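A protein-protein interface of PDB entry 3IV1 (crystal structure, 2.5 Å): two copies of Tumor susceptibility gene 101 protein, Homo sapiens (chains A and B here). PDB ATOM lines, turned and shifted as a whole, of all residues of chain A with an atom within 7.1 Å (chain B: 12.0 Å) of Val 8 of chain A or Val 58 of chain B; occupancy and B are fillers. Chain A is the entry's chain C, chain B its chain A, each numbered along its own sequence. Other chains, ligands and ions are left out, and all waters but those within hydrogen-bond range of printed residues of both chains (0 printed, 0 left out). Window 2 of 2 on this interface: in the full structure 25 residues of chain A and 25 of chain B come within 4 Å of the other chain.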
ATOM      1  N   SER A   3      -9.825 -24.541  20.671  1.00  0.00           N
ATOM      2  CA  SER A   3      -8.704 -24.426  19.746  1.00  0.00           C
ATOM      3  C   SER A   3      -8.901 -23.414  18.603  1.00  0.00           C
ATOM      4  O   SER A   3      -8.195 -23.490  17.600  1.00  0.00           O
ATOM      5  CB  SER A   3      -8.345 -25.807  19.207  1.00  0.00           C
ATOM      6  OG  SER A   3      -7.210 -26.261  19.916  1.00  0.00           O
ATOM      7  N   LEU A   4      -9.805 -22.447  18.766  1.00  0.00           N
ATOM      8  CA  LEU A   4     -10.061 -21.444  17.719  1.00  0.00           C
ATOM      9  C   LEU A   4      -8.880 -20.506  17.415  1.00  0.00           C
ATOM     10  O   LEU A   4      -8.556 -20.336  16.242  1.00  0.00           O
ATOM     11  CB  LEU A   4     -11.386 -20.681  17.934  1.00  0.00           C
ATOM     12  CG  LEU A   4     -12.655 -21.535  18.107  1.00  0.00           C
ATOM     13  CD1 LEU A   4     -13.843 -20.673  18.501  1.00  0.00           C
ATOM     14  CD2 LEU A   4     -12.969 -22.324  16.839  1.00  0.00           C
ATOM     15  N   ILE A   5      -8.220 -19.938  18.457  1.00  0.00           N
ATOM     16  CA  ILE A   5      -7.042 -19.070  18.296  1.00  0.00           C
ATOM     17  C   ILE A   5      -5.937 -19.867  17.594  1.00  0.00           C
ATOM     18  O   ILE A   5      -5.338 -19.362  16.644  1.00  0.00           O
ATOM     19  CB  ILE A   5      -6.545 -18.417  19.635  1.00  0.00           C
ATOM     20  CG1 ILE A   5      -7.552 -17.350  20.150  1.00  0.00           C
ATOM     21  CG2 ILE A   5      -5.113 -17.805  19.463  1.00  0.00           C
ATOM     22  CD1 ILE A   5      -7.234 -16.552  21.486  1.00  0.00           C
ATOM     23  N   SER A   6      -5.686 -21.116  18.040  1.00  0.00           N
ATOM     24  CA  SER A   6      -4.638 -21.958  17.453  1.00  0.00           C
ATOM     25  C   SER A   6      -4.892 -22.296  15.985  1.00  0.00           C
ATOM     26  O   SER A   6      -3.950 -22.222  15.204  1.00  0.00           O
ATOM     27  CB  SER A   6      -4.417 -23.237  18.267  1.00  0.00           C
ATOM     28  OG  SER A   6      -3.895 -22.952  19.552  1.00  0.00           O
ATOM     29  N   ALA A   7      -6.154 -22.638  15.612  1.00  0.00           N
ATOM     30  CA  ALA A   7      -6.564 -22.987  14.241  1.00  0.00           C
ATOM     31  C   ALA A   7      -6.341 -21.806  13.281  1.00  0.00           C
ATOM     32  O   ALA A   7      -5.757 -21.980  12.202  1.00  0.00           O
ATOM     33  CB  ALA A   7      -8.018 -23.404  14.214  1.00  0.00           C
ATOM     34  N   VAL A   8      -6.769 -20.604  13.700  1.00  0.00           N
ATOM     35  CA  VAL A   8      -6.644 -19.354  12.951  1.00  0.00           C
ATOM     36  C   VAL A   8      -5.148 -18.993  12.753  1.00  0.00           C
ATOM     37  O   VAL A   8      -4.739 -18.613  11.657  1.00  0.00           O
ATOM     38  CB  VAL A   8      -7.488 -18.277  13.697  1.00  0.00           C
ATOM     39  CG1 VAL A   8      -6.940 -16.874  13.541  1.00  0.00           C
ATOM     40  CG2 VAL A   8      -8.947 -18.344  13.281  1.00  0.00           C
ATOM     41  N   SER A   9      -4.346 -19.172  13.803  1.00  0.00           N
ATOM     42  CA  SER A   9      -2.911 -18.919  13.809  1.00  0.00           C
ATOM     43  C   SER A   9      -2.158 -19.922  12.912  1.00  0.00           C
ATOM     44  O   SER A   9      -1.295 -19.515  12.122  1.00  0.00           O
ATOM     45  CB  SER A   9      -2.391 -18.921  15.240  1.00  0.00           C
ATOM     46  OG  SER A   9      -1.043 -18.497  15.281  1.00  0.00           O
ATOM     47  N   ASP A  10      -2.530 -21.224  12.989  1.00  0.00           N
ATOM     48  CA  ASP A  10      -1.970 -22.312  12.156  1.00  0.00           C
ATOM     49  C   ASP A  10      -2.266 -22.079  10.663  1.00  0.00           C
ATOM     50  O   ASP A  10      -1.391 -22.281   9.829  1.00  0.00           O
ATOM     51  CB  ASP A  10      -2.548 -23.676  12.571  1.00  0.00           C
ATOM     52  CG  ASP A  10      -2.085 -24.228  13.914  1.00  0.00           C
ATOM     53  OD1 ASP A  10      -1.272 -23.546  14.599  1.00  0.00           O
ATOM     54  OD2 ASP A  10      -2.584 -25.309  14.317  1.00  0.00           O
ATOM     55  N   LYS A  11      -3.498 -21.660  10.343  1.00  0.00           N
ATOM     56  CA  LYS A  11      -3.980 -21.371   8.987  1.00  0.00           C
ATOM     57  C   LYS A  11      -3.128 -20.262   8.341  1.00  0.00           C
ATOM     58  O   LYS A  11      -2.657 -20.437   7.210  1.00  0.00           O
ATOM     59  CB  LYS A  11      -5.482 -20.996   9.009  1.00  0.00           C
ATOM     60  CG  LYS A  11      -6.134 -20.956   7.627  1.00  0.00           C
ATOM     61  CD  LYS A  11      -7.643 -20.768   7.714  1.00  0.00           C
ATOM     62  CE  LYS A  11      -8.268 -20.699   6.346  1.00  0.00           C
ATOM     63  NZ  LYS A  11      -8.669 -19.311   5.981  1.00  0.00           N
ATOM     64  N   LEU A  12      -2.892 -19.154   9.091  1.00  0.00           N
ATOM     65  CA  LEU A  12      -2.065 -18.035   8.644  1.00  0.00           C
ATOM     66  C   LEU A  12      -0.606 -18.486   8.326  1.00  0.00           C
ATOM     67  O   LEU A  12      -0.056 -18.097   7.291  1.00  0.00           O
ATOM     68  CB  LEU A  12      -2.082 -16.883   9.676  1.00  0.00           C
ATOM     69  CG  LEU A  12      -1.207 -15.651   9.306  1.00  0.00           C
ATOM     70  CD1 LEU A  12      -1.687 -15.004   7.947  1.00  0.00           C
ATOM     71  CD2 LEU A  12      -1.203 -14.616  10.440  1.00  0.00           C
ATOM     72  N   ARG A  13      -0.018 -19.315   9.194  1.00  0.00           N
ATOM     73  CA  ARG A  13       1.346 -19.813   9.034  1.00  0.00           C
ATOM     74  C   ARG A  13       1.425 -20.643   7.762  1.00  0.00           C
ATOM     75  O   ARG A  13       2.338 -20.427   6.948  1.00  0.00           O
ATOM     76  CB  ARG A  13       1.751 -20.638  10.266  1.00  0.00           C
ATOM     77  CG  ARG A  13       3.107 -20.309  10.792  1.00  0.00           C
ATOM     78  CD  ARG A  13       3.333 -20.623  12.252  1.00  0.00           C
ATOM     79  NE  ARG A  13       2.784 -21.902  12.681  1.00  0.00           N
ATOM     80  CZ  ARG A  13       1.784 -22.046  13.540  1.00  0.00           C
ATOM     81  NH1 ARG A  13       1.220 -20.988  14.098  1.00  0.00           N
ATOM     82  NH2 ARG A  13       1.349 -23.249  13.856  1.00  0.00           N
ATOM     83  N   ARG A  15      -0.797 -20.489   5.057  1.00  0.00           N
ATOM     84  CA  ARG A  15      -1.051 -19.541   3.971  1.00  0.00           C
ATOM     85  C   ARG A  15       0.225 -18.786   3.632  1.00  0.00           C
ATOM     86  O   ARG A  15       0.516 -18.603   2.454  1.00  0.00           O
ATOM     87  CB  ARG A  15      -2.159 -18.536   4.367  1.00  0.00           C
ATOM     88  CG  ARG A  15      -3.410 -18.593   3.480  1.00  0.00           C
ATOM     89  CD  ARG A  15      -4.439 -17.515   3.837  1.00  0.00           C
ATOM     90  NE  ARG A  15      -5.241 -17.849   5.022  1.00  0.00           N
ATOM     91  CZ  ARG A  15      -5.380 -17.071   6.096  1.00  0.00           C
ATOM     92  NH1 ARG A  15      -4.780 -15.890   6.154  1.00  0.00           N
ATOM     93  NH2 ARG A  15      -6.127 -17.468   7.117  1.00  0.00           N
ATOM     94  N   THR B  49      -0.342  -7.025  -0.433  1.00  0.00           N
ATOM     95  CA  THR B  49      -1.564  -6.372   0.072  1.00  0.00           C
ATOM     96  C   THR B  49      -2.487  -7.394   0.739  1.00  0.00           C
ATOM     97  O   THR B  49      -2.900  -7.180   1.878  1.00  0.00           O
ATOM     98  CB  THR B  49      -2.253  -5.607  -1.083  1.00  0.00           C
ATOM     99  OG1 THR B  49      -1.298  -4.722  -1.644  1.00  0.00           O
ATOM    100  CG2 THR B  49      -3.486  -4.813  -0.641  1.00  0.00           C
ATOM    101  N   ARG B  50      -2.783  -8.505   0.024  1.00  0.00           N
ATOM    102  CA  ARG B  50      -3.629  -9.624   0.460  1.00  0.00           C
ATOM    103  C   ARG B  50      -3.147 -10.174   1.824  1.00  0.00           C
ATOM    104  O   ARG B  50      -3.935 -10.192   2.787  1.00  0.00           O
ATOM    105  CB  ARG B  50      -3.614 -10.717  -0.623  1.00  0.00           C
ATOM    106  CG  ARG B  50      -4.702 -11.777  -0.546  1.00  0.00           C
ATOM    107  CD  ARG B  50      -4.466 -12.900  -1.564  1.00  0.00           C
ATOM    108  NE  ARG B  50      -4.295 -12.423  -2.939  1.00  0.00           N
ATOM    109  CZ  ARG B  50      -3.287 -12.755  -3.743  1.00  0.00           C
ATOM    110  NH1 ARG B  50      -2.331 -13.573  -3.319  1.00  0.00           N
ATOM    111  NH2 ARG B  50      -3.226 -12.270  -4.977  1.00  0.00           N
ATOM    112  N   LEU B  51      -1.842 -10.543   1.912  1.00  0.00           N
ATOM    113  CA  LEU B  51      -1.186 -11.095   3.108  1.00  0.00           C
ATOM    114  C   LEU B  51      -1.125 -10.120   4.248  1.00  0.00           C
ATOM    115  O   LEU B  51      -1.345 -10.521   5.382  1.00  0.00           O
ATOM    116  CB  LEU B  51       0.211 -11.614   2.811  1.00  0.00           C
ATOM    117  CG  LEU B  51       0.314 -13.003   2.206  1.00  0.00           C
ATOM    118  CD1 LEU B  51       1.696 -13.234   1.729  1.00  0.00           C
ATOM    119  CD2 LEU B  51      -0.096 -14.100   3.217  1.00  0.00           C
ATOM    120  N   ASP B  52      -0.876  -8.840   3.959  1.00  0.00           N
ATOM    121  CA  ASP B  52      -0.876  -7.795   4.970  1.00  0.00           C
ATOM    122  C   ASP B  52      -2.286  -7.698   5.621  1.00  0.00           C
ATOM    123  O   ASP B  52      -2.393  -7.637   6.848  1.00  0.00           O
ATOM    124  CB  ASP B  52      -0.445  -6.459   4.351  1.00  0.00           C
ATOM    125  CG  ASP B  52      -0.114  -5.419   5.393  1.00  0.00           C
ATOM    126  OD1 ASP B  52       0.992  -5.496   5.985  1.00  0.00           O
ATOM    127  OD2 ASP B  52      -0.982  -4.567   5.670  1.00  0.00           O
ATOM    128  N   GLN B  53      -3.351  -7.758   4.791  1.00  0.00           N
ATOM    129  CA  GLN B  53      -4.735  -7.752   5.229  1.00  0.00           C
ATOM    130  C   GLN B  53      -5.076  -9.042   6.001  1.00  0.00           C
ATOM    131  O   GLN B  53      -5.787  -8.980   7.010  1.00  0.00           O
ATOM    132  CB  GLN B  53      -5.672  -7.573   4.020  1.00  0.00           C
ATOM    133  CG  GLN B  53      -6.538  -6.328   4.119  1.00  0.00           C
ATOM    134  CD  GLN B  53      -7.619  -6.492   5.174  1.00  0.00           C
ATOM    135  OE1 GLN B  53      -8.565  -7.270   5.010  1.00  0.00           O
ATOM    136  NE2 GLN B  53      -7.478  -5.802   6.305  1.00  0.00           N
ATOM    137  N   GLU B  54      -4.553 -10.202   5.537  1.00  0.00           N
ATOM    138  CA  GLU B  54      -4.775 -11.504   6.180  1.00  0.00           C
ATOM    139  C   GLU B  54      -4.160 -11.543   7.572  1.00  0.00           C
ATOM    140  O   GLU B  54      -4.831 -12.021   8.493  1.00  0.00           O
ATOM    141  CB  GLU B  54      -4.289 -12.657   5.304  1.00  0.00           C
ATOM    142  CG  GLU B  54      -5.288 -13.005   4.204  1.00  0.00           C
ATOM    143  CD  GLU B  54      -4.808 -13.880   3.058  1.00  0.00           C
ATOM    144  OE1 GLU B  54      -3.630 -14.304   3.079  1.00  0.00           O
ATOM    145  OE2 GLU B  54      -5.609 -14.123   2.126  1.00  0.00           O
ATOM    146  N   VAL B  55      -2.959 -10.935   7.765  1.00  0.00           N
ATOM    147  CA  VAL B  55      -2.349 -10.828   9.094  1.00  0.00           C
ATOM    148  C   VAL B  55      -3.245  -9.969  10.041  1.00  0.00           C
ATOM    149  O   VAL B  55      -3.517 -10.401  11.160  1.00  0.00           O
ATOM    150  CB  VAL B  55      -0.863 -10.361   9.063  1.00  0.00           C
ATOM    151  CG1 VAL B  55      -0.322 -10.146  10.479  1.00  0.00           C
ATOM    152  CG2 VAL B  55       0.018 -11.354   8.292  1.00  0.00           C
ATOM    153  N   ALA B  56      -3.723  -8.783   9.568  1.00  0.00           N
ATOM    154  CA  ALA B  56      -4.622  -7.886  10.302  1.00  0.00           C
ATOM    155  C   ALA B  56      -5.932  -8.575  10.686  1.00  0.00           C
ATOM    156  O   ALA B  56      -6.400  -8.414  11.810  1.00  0.00           O
ATOM    157  CB  ALA B  56      -4.914  -6.641   9.483  1.00  0.00           C
ATOM    158  N   GLU B  57      -6.475  -9.396   9.781  1.00  0.00           N
ATOM    159  CA  GLU B  57      -7.714 -10.157   9.994  1.00  0.00           C
ATOM    160  C   GLU B  57      -7.575 -11.178  11.140  1.00  0.00           C
ATOM    161  O   GLU B  57      -8.464 -11.275  11.985  1.00  0.00           O
ATOM    162  CB  GLU B  57      -8.164 -10.853   8.698  1.00  0.00           C
ATOM    163  CG  GLU B  57      -8.908  -9.966   7.717  1.00  0.00           C
ATOM    164  CD  GLU B  57      -9.421 -10.637   6.454  1.00  0.00           C
ATOM    165  OE1 GLU B  57      -9.470 -11.890   6.416  1.00  0.00           O
ATOM    166  OE2 GLU B  57      -9.739  -9.903   5.487  1.00  0.00           O
ATOM    167  N   VAL B  58      -6.448 -11.916  11.168  1.00  0.00           N
ATOM    168  CA  VAL B  58      -6.109 -12.894  12.195  1.00  0.00           C
ATOM    169  C   VAL B  58      -5.920 -12.161  13.545  1.00  0.00           C
ATOM    170  O   VAL B  58      -6.536 -12.564  14.546  1.00  0.00           O
ATOM    171  CB  VAL B  58      -4.898 -13.763  11.760  1.00  0.00           C
ATOM    172  CG1 VAL B  58      -4.276 -14.549  12.934  1.00  0.00           C
ATOM    173  CG2 VAL B  58      -5.301 -14.708  10.620  1.00  0.00           C
ATOM    174  N   ASP B  59      -5.154 -11.036  13.541  1.00  0.00           N
ATOM    175  CA  ASP B  59      -4.989 -10.185  14.732  1.00  0.00           C
ATOM    176  C   ASP B  59      -6.366  -9.820  15.330  1.00  0.00           C
ATOM    177  O   ASP B  59      -6.562 -10.021  16.530  1.00  0.00           O
ATOM    178  CB  ASP B  59      -4.213  -8.903  14.399  1.00  0.00           C
ATOM    179  CG  ASP B  59      -2.704  -9.073  14.259  1.00  0.00           C
ATOM    180  OD1 ASP B  59      -2.156 -10.025  14.861  1.00  0.00           O
ATOM    181  OD2 ASP B  59      -2.053  -8.181  13.642  1.00  0.00           O
ATOM    182  N   LYS B  60      -7.325  -9.352  14.489  1.00  0.00           N
ATOM    183  CA  LYS B  60      -8.695  -9.011  14.924  1.00  0.00           C
ATOM    184  C   LYS B  60      -9.462 -10.244  15.414  1.00  0.00           C
ATOM    185  O   LYS B  60     -10.094 -10.166  16.459  1.00  0.00           O
ATOM    186  CB  LYS B  60      -9.481  -8.239  13.857  1.00  0.00           C
ATOM    187  CG  LYS B  60     -10.747  -7.593  14.415  1.00  0.00           C
ATOM    188  CD  LYS B  60     -11.258  -6.467  13.541  1.00  0.00           C
ATOM    189  CE  LYS B  60     -12.602  -5.958  14.009  1.00  0.00           C
ATOM    190  NZ  LYS B  60     -12.492  -5.112  15.229  1.00  0.00           N
ATOM    191  N   ASN B  61      -9.360 -11.387  14.697  1.00  0.00           N
ATOM    192  CA  ASN B  61      -9.991 -12.646  15.106  1.00  0.00           C
ATOM    193  C   ASN B  61      -9.576 -13.052  16.509  1.00  0.00           C
ATOM    194  O   ASN B  61     -10.444 -13.287  17.352  1.00  0.00           O
ATOM    195  CB  ASN B  61      -9.674 -13.760  14.111  1.00  0.00           C
ATOM    196  CG  ASN B  61     -10.531 -13.689  12.869  1.00  0.00           C
ATOM    197  OD1 ASN B  61     -11.684 -13.268  12.909  1.00  0.00           O
ATOM    198  ND2 ASN B  61     -10.026 -14.183  11.758  1.00  0.00           N
ATOM    199  N   ILE B  62      -8.266 -13.083  16.780  1.00  0.00           N
ATOM    200  CA  ILE B  62      -7.754 -13.446  18.085  1.00  0.00           C
ATOM    201  C   ILE B  62      -8.171 -12.438  19.150  1.00  0.00           C
ATOM    202  O   ILE B  62      -8.540 -12.859  20.246  1.00  0.00           O
ATOM    203  CB  ILE B  62      -6.250 -13.932  18.142  1.00  0.00           C
ATOM    204  CG1 ILE B  62      -5.290 -12.915  18.669  1.00  0.00           C
ATOM    205  CG2 ILE B  62      -5.733 -14.679  16.903  1.00  0.00           C
ATOM    206  CD1 ILE B  62      -4.979 -13.178  19.991  1.00  0.00           C
ATOM    207  N   GLU B  63      -8.165 -11.126  18.820  1.00  0.00           N
ATOM    208  CA  GLU B  63      -8.604 -10.081  19.741  1.00  0.00           C
ATOM    209  C   GLU B  63     -10.074 -10.312  20.134  1.00  0.00           C
ATOM    210  O   GLU B  63     -10.416 -10.173  21.316  1.00  0.00           O
ATOM    211  CB  GLU B  63      -8.458  -8.689  19.120  1.00  0.00           C
ATOM    212  CG  GLU B  63      -7.099  -8.035  19.269  1.00  0.00           C
ATOM    213  CD  GLU B  63      -7.050  -6.698  18.554  1.00  0.00           C
ATOM    214  OE1 GLU B  63      -6.144  -6.516  17.710  1.00  0.00           O
ATOM    215  OE2 GLU B  63      -7.939  -5.849  18.804  1.00  0.00           O
ATOM    216  N   LEU B  64     -10.931 -10.718  19.165  1.00  0.00           N
ATOM    217  CA  LEU B  64     -12.348 -11.009  19.429  1.00  0.00           C
ATOM    218  C   LEU B  64     -12.532 -12.247  20.317  1.00  0.00           C
ATOM    219  O   LEU B  64     -13.367 -12.236  21.219  1.00  0.00           O
ATOM    220  CB  LEU B  64     -13.145 -11.136  18.110  1.00  0.00           C
ATOM    221  CG  LEU B  64     -13.526  -9.815  17.440  1.00  0.00           C
ATOM    222  CD1 LEU B  64     -13.679  -9.999  15.947  1.00  0.00           C
ATOM    223  CD2 LEU B  64     -14.793  -9.231  18.014  1.00  0.00           C
ATOM    224  N   LEU B  65     -11.705 -13.285  20.091  1.00  0.00           N
ATOM    225  CA  LEU B  65     -11.733 -14.518  20.878  1.00  0.00           C
ATOM    226  C   LEU B  65     -11.235 -14.284  22.303  1.00  0.00           C
ATOM    227  O   LEU B  65     -11.772 -14.877  23.247  1.00  0.00           O
ATOM    228  CB  LEU B  65     -10.986 -15.681  20.188  1.00  0.00           C
ATOM    229  CG  LEU B  65     -11.588 -16.176  18.862  1.00  0.00           C
ATOM    230  CD1 LEU B  65     -10.586 -16.995  18.076  1.00  0.00           C
ATOM    231  CD2 LEU B  65     -12.870 -16.964  19.073  1.00  0.00           C
ATOM    232  N   LYS B  66     -10.272 -13.365  22.464  1.00  0.00           N
ATOM    233  CA  LYS B  66      -9.754 -12.998  23.785  1.00  0.00           C
ATOM    234  C   LYS B  66     -10.830 -12.243  24.573  1.00  0.00           C
ATOM    235  O   LYS B  66     -11.090 -12.579  25.723  1.00  0.00           O
ATOM    236  CB  LYS B  66      -8.471 -12.163  23.660  1.00  0.00           C
ATOM    237  CG  LYS B  66      -7.245 -12.987  23.347  1.00  0.00           C
ATOM    238  CD  LYS B  66      -5.982 -12.153  23.426  1.00  0.00           C
ATOM    239  CE  LYS B  66      -4.745 -13.015  23.477  1.00  0.00           C
ATOM    240  NZ  LYS B  66      -3.536 -12.257  23.060  1.00  0.00           N
ATOM    241  N   LYS B  67     -11.493 -11.266  23.931  1.00  0.00           N
ATOM    242  CA  LYS B  67     -12.570 -10.488  24.530  1.00  0.00           C
ATOM    243  C   LYS B  67     -13.655 -11.446  25.036  1.00  0.00           C
ATOM    244  O   LYS B  67     -14.152 -11.284  26.157  1.00  0.00           O
ATOM    245  CB  LYS B  67     -13.162  -9.510  23.517  1.00  0.00           C
ATOM    246  CG  LYS B  67     -12.715  -8.070  23.731  1.00  0.00           C
ATOM    247  CD  LYS B  67     -13.210  -7.161  22.586  1.00  0.00           C
ATOM    248  CE  LYS B  67     -12.154  -6.274  21.954  1.00  0.00           C
ATOM    249  NZ  LYS B  67     -11.583  -5.289  22.915  1.00  0.00           N
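The guanidinium group of Arg 15 of chain A is in salt-bridge range of the side-chain carboxylate of Glu 54 of chain B (3.6 Å).
Among the printed residues, merely in contact across the chains: Val 8 of chain A with Val 58 of chain B, Ile 5 of chain A with Leu 65 of chain B, Leu 4 of chain A with Leu 65 of chain B and Leu 12 of chain A with Val 58 of chain B.
Of chain B, only Val 58 (3.6 Å) comes within 4 Å of Val 8 of chain A. Of chain A, only Val 8 (3.6 Å) and Leu 12 (3.96 Å) come within 4 Å of Val 58 of chain B. Leu 4 of chain A touches just one residue of chain B: Leu 65. No residue of chain B comes within 4 Å of Ser 6 of chain A. No residue of chain B comes within 4 Å of Ala 7 of chain A. No residue of chain B comes within 4 Å of Ser 9 of chain A. No residue of chain B comes within 4 Å of Asp 10 of chain A. Leu 12 of chain A touches one residue of chain B. Of the printed residues of chain A, Glu 54 of chain B touches Arg 15 (3.4 Å). Of the printed residues of chain B, Arg 15 of chain A touches Glu 54. Leu 51 of chain B touches none of the printed residues of chain A. The nearest printed residue of chain B that does not touch Val 8 of chain A is Asn 61 of chain B (4.2 Å). The nearest printed residue of chain A that does not touch Glu 54 of chain B is Leu 12 of chain A (4.3 Å).
Of the 19 printed residues of chain B, 3 touch a printed residue of chain A. Hydrophobic or aromatic side chains of chain B that line the printed part of chain A: Val 58 and Leu 65. Of the 12 printed residues of chain A, 5 touch a printed residue of chain B. Printed residues of chain A that touch a printed residue of chain B: Leu 4, Ile 5, Val 8, Leu 12 and Arg 15. Hydrophobic or aromatic side chains of chain A that line the printed part of chain B: Leu 4, Ile 5, Val 8 and Leu 12.
No position is printed for both chains. Of the 5 pairs that touch across the chains among the printed residues, none has its exchanged pair printed and touching as well.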
